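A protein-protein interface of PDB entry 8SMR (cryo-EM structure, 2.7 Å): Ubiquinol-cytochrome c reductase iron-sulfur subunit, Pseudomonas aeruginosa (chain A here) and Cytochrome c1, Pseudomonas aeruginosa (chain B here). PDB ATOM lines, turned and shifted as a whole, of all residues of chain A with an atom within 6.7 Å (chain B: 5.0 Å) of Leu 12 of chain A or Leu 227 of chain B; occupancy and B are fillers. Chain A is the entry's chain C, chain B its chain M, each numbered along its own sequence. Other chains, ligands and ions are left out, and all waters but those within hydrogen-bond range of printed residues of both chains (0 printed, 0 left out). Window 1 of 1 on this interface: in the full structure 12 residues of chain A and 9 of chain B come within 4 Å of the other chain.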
ATOM      1  N   GLY A   7       2.626  20.142  14.256  1.00  0.00           N
ATOM      2  CA  GLY A   7       3.579  20.211  15.353  1.00  0.00           C
ATOM      3  C   GLY A   7       3.027  19.627  16.639  1.00  0.00           C
ATOM      4  O   GLY A   7       3.661  18.782  17.277  1.00  0.00           O
ATOM      5  N   ARG A   8       1.829  20.064  17.035  1.00  0.00           N
ATOM      6  CA  ARG A   8       1.218  19.529  18.246  1.00  0.00           C
ATOM      7  C   ARG A   8       0.900  18.049  18.096  1.00  0.00           C
ATOM      8  O   ARG A   8       1.076  17.275  19.043  1.00  0.00           O
ATOM      9  CB  ARG A   8      -0.046  20.308  18.605  1.00  0.00           C
ATOM     10  CG  ARG A   8      -0.582  19.965  19.987  1.00  0.00           C
ATOM     11  CD  ARG A   8      -1.438  21.078  20.573  1.00  0.00           C
ATOM     12  NE  ARG A   8      -2.123  20.671  21.797  1.00  0.00           N
ATOM     13  CZ  ARG A   8      -1.521  20.282  22.913  1.00  0.00           C
ATOM     14  NH1 ARG A   8      -0.203  20.292  23.034  1.00  0.00           N
ATOM     15  NH2 ARG A   8      -2.262  19.881  23.942  1.00  0.00           N
ATOM     16  N   ARG A   9       0.417  17.636  16.924  1.00  0.00           N
ATOM     17  CA  ARG A   9       0.121  16.224  16.710  1.00  0.00           C
ATOM     18  C   ARG A   9       1.372  15.375  16.901  1.00  0.00           C
ATOM     19  O   ARG A   9       1.348  14.362  17.610  1.00  0.00           O
ATOM     20  CB  ARG A   9      -0.460  16.016  15.312  1.00  0.00           C
ATOM     21  CG  ARG A   9      -1.547  14.956  15.239  1.00  0.00           C
ATOM     22  CD  ARG A   9      -2.346  15.077  13.954  1.00  0.00           C
ATOM     23  NE  ARG A   9      -3.609  15.776  14.160  1.00  0.00           N
ATOM     24  CZ  ARG A   9      -4.720  15.547  13.474  1.00  0.00           C
ATOM     25  NH1 ARG A   9      -4.765  14.648  12.504  1.00  0.00           N
ATOM     26  NH2 ARG A   9      -5.816  16.242  13.765  1.00  0.00           N
ATOM     27  N   ARG A  10       2.480  15.779  16.278  1.00  0.00           N
ATOM     28  CA  ARG A  10       3.717  15.016  16.399  1.00  0.00           C
ATOM     29  C   ARG A  10       4.231  15.024  17.831  1.00  0.00           C
ATOM     30  O   ARG A  10       4.668  13.985  18.341  1.00  0.00           O
ATOM     31  CB  ARG A  10       4.777  15.573  15.449  1.00  0.00           C
ATOM     32  CG  ARG A  10       4.920  14.782  14.156  1.00  0.00           C
ATOM     33  CD  ARG A  10       5.917  15.420  13.198  1.00  0.00           C
ATOM     34  NE  ARG A  10       6.960  16.168  13.896  1.00  0.00           N
ATOM     35  CZ  ARG A  10       7.048  17.491  13.946  1.00  0.00           C
ATOM     36  NH1 ARG A  10       6.157  18.271  13.354  1.00  0.00           N
ATOM     37  NH2 ARG A  10       8.057  18.047  14.610  1.00  0.00           N
ATOM     38  N   PHE A  11       4.195  16.181  18.498  1.00  0.00           N
ATOM     39  CA  PHE A  11       4.668  16.232  19.876  1.00  0.00           C
ATOM     40  C   PHE A  11       3.835  15.328  20.772  1.00  0.00           C
ATOM     41  O   PHE A  11       4.382  14.602  21.608  1.00  0.00           O
ATOM     42  CB  PHE A  11       4.631  17.662  20.411  1.00  0.00           C
ATOM     43  CG  PHE A  11       4.634  17.735  21.912  1.00  0.00           C
ATOM     44  CD1 PHE A  11       5.796  17.492  22.628  1.00  0.00           C
ATOM     45  CD2 PHE A  11       3.476  18.028  22.609  1.00  0.00           C
ATOM     46  CE1 PHE A  11       5.802  17.549  24.008  1.00  0.00           C
ATOM     47  CE2 PHE A  11       3.476  18.087  23.991  1.00  0.00           C
ATOM     48  CZ  PHE A  11       4.642  17.847  24.689  1.00  0.00           C
ATOM     49  N   LEU A  12       2.509  15.368  20.625  1.00  0.00           N
ATOM     50  CA  LEU A  12       1.652  14.533  21.454  1.00  0.00           C
ATOM     51  C   LEU A  12       1.863  13.056  21.163  1.00  0.00           C
ATOM     52  O   LEU A  12       1.892  12.246  22.093  1.00  0.00           O
ATOM     53  CB  LEU A  12       0.187  14.914  21.245  1.00  0.00           C
ATOM     54  CG  LEU A  12      -0.299  16.098  22.084  1.00  0.00           C
ATOM     55  CD1 LEU A  12      -1.600  16.650  21.532  1.00  0.00           C
ATOM     56  CD2 LEU A  12      -0.462  15.693  23.542  1.00  0.00           C
ATOM     57  N   VAL A  13       2.023  12.684  19.892  1.00  0.00           N
ATOM     58  CA  VAL A  13       2.273  11.283  19.566  1.00  0.00           C
ATOM     59  C   VAL A  13       3.582  10.824  20.193  1.00  0.00           C
ATOM     60  O   VAL A  13       3.651   9.761  20.820  1.00  0.00           O
ATOM     61  CB  VAL A  13       2.272  11.078  18.040  1.00  0.00           C
ATOM     62  CG1 VAL A  13       2.770   9.684  17.690  1.00  0.00           C
ATOM     63  CG2 VAL A  13       0.878  11.295  17.478  1.00  0.00           C
ATOM     64  N   ALA A  14       4.638  11.628  20.047  1.00  0.00           N
ATOM     65  CA  ALA A  14       5.935  11.253  20.597  1.00  0.00           C
ATOM     66  C   ALA A  14       5.886  11.164  22.118  1.00  0.00           C
ATOM     67  O   ALA A  14       6.433  10.229  22.712  1.00  0.00           O
ATOM     68  CB  ALA A  14       7.000  12.254  20.153  1.00  0.00           C
ATOM     69  N   ALA A  15       5.236  12.132  22.767  1.00  0.00           N
ATOM     70  CA  ALA A  15       5.167  12.133  24.223  1.00  0.00           C
ATOM     71  C   ALA A  15       4.350  10.958  24.737  1.00  0.00           C
ATOM     72  O   ALA A  15       4.739  10.305  25.712  1.00  0.00           O
ATOM     73  CB  ALA A  15       4.576  13.453  24.716  1.00  0.00           C
ATOM     74  N   THR A  16       3.212  10.674  24.101  1.00  0.00           N
ATOM     75  CA  THR A  16       2.413   9.526  24.503  1.00  0.00           C
ATOM     76  C   THR A  16       3.187   8.232  24.304  1.00  0.00           C
ATOM     77  O   THR A  16       3.140   7.340  25.154  1.00  0.00           O
ATOM     78  CB  THR A  16       1.103   9.493  23.717  1.00  0.00           C
ATOM     79  OG1 THR A  16       0.581  10.822  23.599  1.00  0.00           O
ATOM     80  CG2 THR A  16       0.080   8.613  24.417  1.00  0.00           C
ATOM     81  N   SER A  17       3.920   8.117  23.194  1.00  0.00           N
ATOM     82  CA  SER A  17       4.712   6.916  22.959  1.00  0.00           C
ATOM     83  C   SER A  17       5.806   6.762  24.008  1.00  0.00           C
ATOM     84  O   SER A  17       6.042   5.658  24.507  1.00  0.00           O
ATOM     85  CB  SER A  17       5.318   6.959  21.557  1.00  0.00           C
ATOM     86  OG  SER A  17       4.350   6.634  20.575  1.00  0.00           O
ATOM     87  N   VAL B 222      -3.366  12.092  30.850  1.00  0.00           N
ATOM     88  CA  VAL B 222      -3.433  13.433  30.287  1.00  0.00           C
ATOM     89  C   VAL B 222      -2.844  13.471  28.886  1.00  0.00           C
ATOM     90  O   VAL B 222      -3.443  14.062  27.982  1.00  0.00           O
ATOM     91  CB  VAL B 222      -2.713  14.435  31.209  1.00  0.00           C
ATOM     92  CG1 VAL B 222      -2.440  15.742  30.476  1.00  0.00           C
ATOM     93  CG2 VAL B 222      -3.533  14.679  32.464  1.00  0.00           C
ATOM     94  N   PHE B 223      -1.685  12.851  28.680  1.00  0.00           N
ATOM     95  CA  PHE B 223      -1.086  12.775  27.355  1.00  0.00           C
ATOM     96  C   PHE B 223      -1.940  11.961  26.392  1.00  0.00           C
ATOM     97  O   PHE B 223      -2.118  12.360  25.236  1.00  0.00           O
ATOM     98  CB  PHE B 223       0.316  12.171  27.453  1.00  0.00           C
ATOM     99  CG  PHE B 223       1.370  13.164  27.839  1.00  0.00           C
ATOM    100  CD1 PHE B 223       1.742  14.174  26.969  1.00  0.00           C
ATOM    101  CD2 PHE B 223       1.978  13.099  29.080  1.00  0.00           C
ATOM    102  CE1 PHE B 223       2.709  15.092  27.326  1.00  0.00           C
ATOM    103  CE2 PHE B 223       2.943  14.014  29.440  1.00  0.00           C
ATOM    104  CZ  PHE B 223       3.309  15.012  28.564  1.00  0.00           C
ATOM    105  N   ALA B 224      -2.472  10.824  26.844  1.00  0.00           N
ATOM    106  CA  ALA B 224      -3.372  10.047  26.000  1.00  0.00           C
ATOM    107  C   ALA B 224      -4.641  10.829  25.690  1.00  0.00           C
ATOM    108  O   ALA B 224      -5.113  10.833  24.547  1.00  0.00           O
ATOM    109  CB  ALA B 224      -3.713   8.721  26.678  1.00  0.00           C
ATOM    110  N   TYR B 225      -5.212  11.494  26.697  1.00  0.00           N
ATOM    111  CA  TYR B 225      -6.424  12.274  26.470  1.00  0.00           C
ATOM    112  C   TYR B 225      -6.165  13.424  25.507  1.00  0.00           C
ATOM    113  O   TYR B 225      -6.965  13.676  24.600  1.00  0.00           O
ATOM    114  CB  TYR B 225      -6.964  12.801  27.799  1.00  0.00           C
ATOM    115  CG  TYR B 225      -8.146  13.728  27.642  1.00  0.00           C
ATOM    116  CD1 TYR B 225      -7.984  15.105  27.694  1.00  0.00           C
ATOM    117  CD2 TYR B 225      -9.424  13.226  27.441  1.00  0.00           C
ATOM    118  CE1 TYR B 225      -9.062  15.957  27.551  1.00  0.00           C
ATOM    119  CE2 TYR B 225     -10.508  14.069  27.297  1.00  0.00           C
ATOM    120  CZ  TYR B 225     -10.321  15.433  27.353  1.00  0.00           C
ATOM    121  OH  TYR B 225     -11.399  16.276  27.210  1.00  0.00           O
ATOM    122  N   LEU B 226      -5.052  14.137  25.691  1.00  0.00           N
ATOM    123  CA  LEU B 226      -4.720  15.229  24.782  1.00  0.00           C
ATOM    124  C   LEU B 226      -4.459  14.711  23.374  1.00  0.00           C
ATOM    125  O   LEU B 226      -4.900  15.318  22.391  1.00  0.00           O
ATOM    126  CB  LEU B 226      -3.506  15.996  25.304  1.00  0.00           C
ATOM    127  CG  LEU B 226      -3.742  16.933  26.492  1.00  0.00           C
ATOM    128  CD1 LEU B 226      -2.436  17.578  26.919  1.00  0.00           C
ATOM    129  CD2 LEU B 226      -4.778  17.995  26.163  1.00  0.00           C
ATOM    130  N   LEU B 227      -3.742  13.592  23.255  1.00  0.00           N
ATOM    131  CA  LEU B 227      -3.487  13.019  21.938  1.00  0.00           C
ATOM    132  C   LEU B 227      -4.792  12.659  21.241  1.00  0.00           C
ATOM    133  O   LEU B 227      -4.966  12.937  20.049  1.00  0.00           O
ATOM    134  CB  LEU B 227      -2.587  11.790  22.068  1.00  0.00           C
ATOM    135  CG  LEU B 227      -2.429  10.917  20.820  1.00  0.00           C
ATOM    136  CD1 LEU B 227      -1.785  11.707  19.694  1.00  0.00           C
ATOM    137  CD2 LEU B 227      -1.613   9.675  21.134  1.00  0.00           C
ATOM    138  N   LYS B 228      -5.723  12.040  21.968  1.00  0.00           N
ATOM    139  CA  LYS B 228      -7.024  11.730  21.387  1.00  0.00           C
ATOM    140  C   LYS B 228      -7.760  13.000  20.988  1.00  0.00           C
ATOM    141  O   LYS B 228      -8.360  13.068  19.908  1.00  0.00           O
ATOM    142  CB  LYS B 228      -7.859  10.916  22.375  1.00  0.00           C
ATOM    143  CG  LYS B 228      -9.181  10.419  21.814  1.00  0.00           C
ATOM    144  CD  LYS B 228     -10.329  11.358  22.147  1.00  0.00           C
ATOM    145  CE  LYS B 228     -11.635  10.870  21.550  1.00  0.00           C
ATOM    146  NZ  LYS B 228     -12.649  11.957  21.470  1.00  0.00           N
ATOM    147  N   ARG B 229      -7.727  14.020  21.847  1.00  0.00           N
ATOM    148  CA  ARG B 229      -8.414  15.268  21.539  1.00  0.00           C
ATOM    149  C   ARG B 229      -7.818  15.928  20.302  1.00  0.00           C
ATOM    150  O   ARG B 229      -8.548  16.481  19.470  1.00  0.00           O
ATOM    151  CB  ARG B 229      -8.346  16.208  22.742  1.00  0.00           C
ATOM    152  CG  ARG B 229      -8.909  17.596  22.488  1.00  0.00           C
ATOM    153  CD  ARG B 229      -8.903  18.433  23.755  1.00  0.00           C
ATOM    154  NE  ARG B 229      -9.210  19.833  23.488  1.00  0.00           N
ATOM    155  CZ  ARG B 229      -8.318  20.743  23.120  1.00  0.00           C
ATOM    156  NH1 ARG B 229      -7.040  20.437  22.962  1.00  0.00           N
ATOM    157  NH2 ARG B 229      -8.719  21.993  22.903  1.00  0.00           N
ATOM    158  N   GLU B 230      -6.491  15.883  20.164  1.00  0.00           N
ATOM    159  CA  GLU B 230      -5.848  16.479  18.998  1.00  0.00           C
ATOM    160  C   GLU B 230      -6.289  15.796  17.711  1.00  0.00           C
ATOM    161  O   GLU B 230      -6.587  16.465  16.714  1.00  0.00           O
ATOM    162  CB  GLU B 230      -4.329  16.401  19.147  1.00  0.00           C
ATOM    163  CG  GLU B 230      -3.554  17.121  18.055  1.00  0.00           C
ATOM    164  CD  GLU B 230      -3.862  18.603  17.994  1.00  0.00           C
ATOM    165  OE1 GLU B 230      -3.941  19.240  19.066  1.00  0.00           O
ATOM    166  OE2 GLU B 230      -4.027  19.131  16.875  1.00  0.00           O
ATOM    167  N   TYR B 231      -6.336  14.463  17.709  1.00  0.00           N
ATOM    168  CA  TYR B 231      -6.653  13.741  16.483  1.00  0.00           C
ATOM    169  C   TYR B 231      -8.124  13.866  16.110  1.00  0.00           C
ATOM    170  O   TYR B 231      -8.455  13.916  14.921  1.00  0.00           O
ATOM    171  CB  TYR B 231      -6.270  12.269  16.625  1.00  0.00           C
ATOM    172  CG  TYR B 231      -4.916  11.939  16.044  1.00  0.00           C
ATOM    173  CD1 TYR B 231      -4.777  11.628  14.699  1.00  0.00           C
ATOM    174  CD2 TYR B 231      -3.778  11.940  16.837  1.00  0.00           C
ATOM    175  CE1 TYR B 231      -3.542  11.327  14.161  1.00  0.00           C
ATOM    176  CE2 TYR B 231      -2.539  11.640  16.306  1.00  0.00           C
ATOM    177  CZ  TYR B 231      -2.428  11.334  14.968  1.00  0.00           C
ATOM    178  OH  TYR B 231      -1.196  11.034  14.433  1.00  0.00           O
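NH2 of Arg 9 of chain A lies within hydrogen-bond range of O of Glu 230 of chain B, 3.1 Å away.
NE of Arg 8 of chain A lies within salt-bridge range of OE1 of Glu 230 of chain B.
The backbone carbonyl oxygen (O) of Val 13 of chain A is in hydrogen-bond range of the side-chain hydroxyl (OG) of Ser 17 of chain A (3.2 Å).
OG1 of Thr 16 of chain A lies within hydrogen-bond range of O of Leu 12 of chain A.
Among the printed residues, merely in contact across the chains: Arg 8 of chain A with Leu 226 of chain B (3.8 Å), Arg 9 of chain A with Tyr 231 of chain B (3.6 Å), Leu 12 of chain A with Leu 226 of chain B (3.5 Å), Leu 12 of chain A with Leu 227 of chain B (3.9 Å), Leu 12 of chain A with Glu 230 of chain B (3.6 Å), Val 13 of chain A with Leu 227 of chain B (3.5 Å), Val 13 of chain A with Tyr 231 of chain B (3.6 Å), Ala 15 of chain A with Phe 223 of chain B (3.6 Å), Thr 16 of chain A with Phe 223 of chain B (3.5 Å) and Thr 16 of chain A with Leu 227 of chain B (3.5 Å).
Leu 12 of chain A touches just these residues of chain B: Leu 226, Leu 227 and Glu 230.
Of the printed residues of chain A, Leu 227 of chain B touches Leu 12 (3.9 Å), Val 13 (3.5 Å) and Thr 16 (3.5 Å).
Printed residues of chain B within 4 Å of Thr 16 of chain A: Phe 223 and Leu 227.
Printed residues of chain A within 4 Å of Glu 230 of chain B: Arg 8 (3.5 Å), Arg 9 (3.1 Å) and Leu 12 (3.6 Å).
Of the printed residues of chain A, Tyr 231 of chain B touches Arg 9 and Val 13.
Of the printed residues of chain B, Arg 9 of chain A touches Glu 230 (3.1 Å) and Tyr 231 (3.6 Å).
Printed residues of chain A within 4 Å of Phe 223 of chain B: Ala 15 (3.6 Å) and Thr 16 (3.5 Å).
Val 222 of chain B touches none of the printed residues of chain A.
Ala 224 of chain B touches none of the printed residues of chain A.
The nearest residue of chain B that does not touch Leu 12 of chain A is Phe 223 of chain B (4.1 Å).
Of the 10 printed residues of chain B, 5 touch a printed residue of chain A.
Printed residues of chain B that touch a printed residue of chain A: Phe 223, Leu 226, Leu 227, Glu 230 and Tyr 231.
Hydrophobic or aromatic side chains of chain B within 4 Å of the printed part of chain A: Phe 223, Leu 226, Leu 227 and Tyr 231.
Of the 11 printed residues of chain A, 6 touch a printed residue of chain B.
Hydrophobic or aromatic side chains of chain A within 4 Å of the printed part of chain B: Leu 12, Val 13 and Ala 15.
Among the printed residues, 12 pairs touch across the chains.
Among the printed residues, Asp or Glu carboxylates within 4 Å of a Lys or Arg side-chain nitrogen of the other chain: Arg 8 of chain A with Glu 230 of chain B (3.6 Å).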
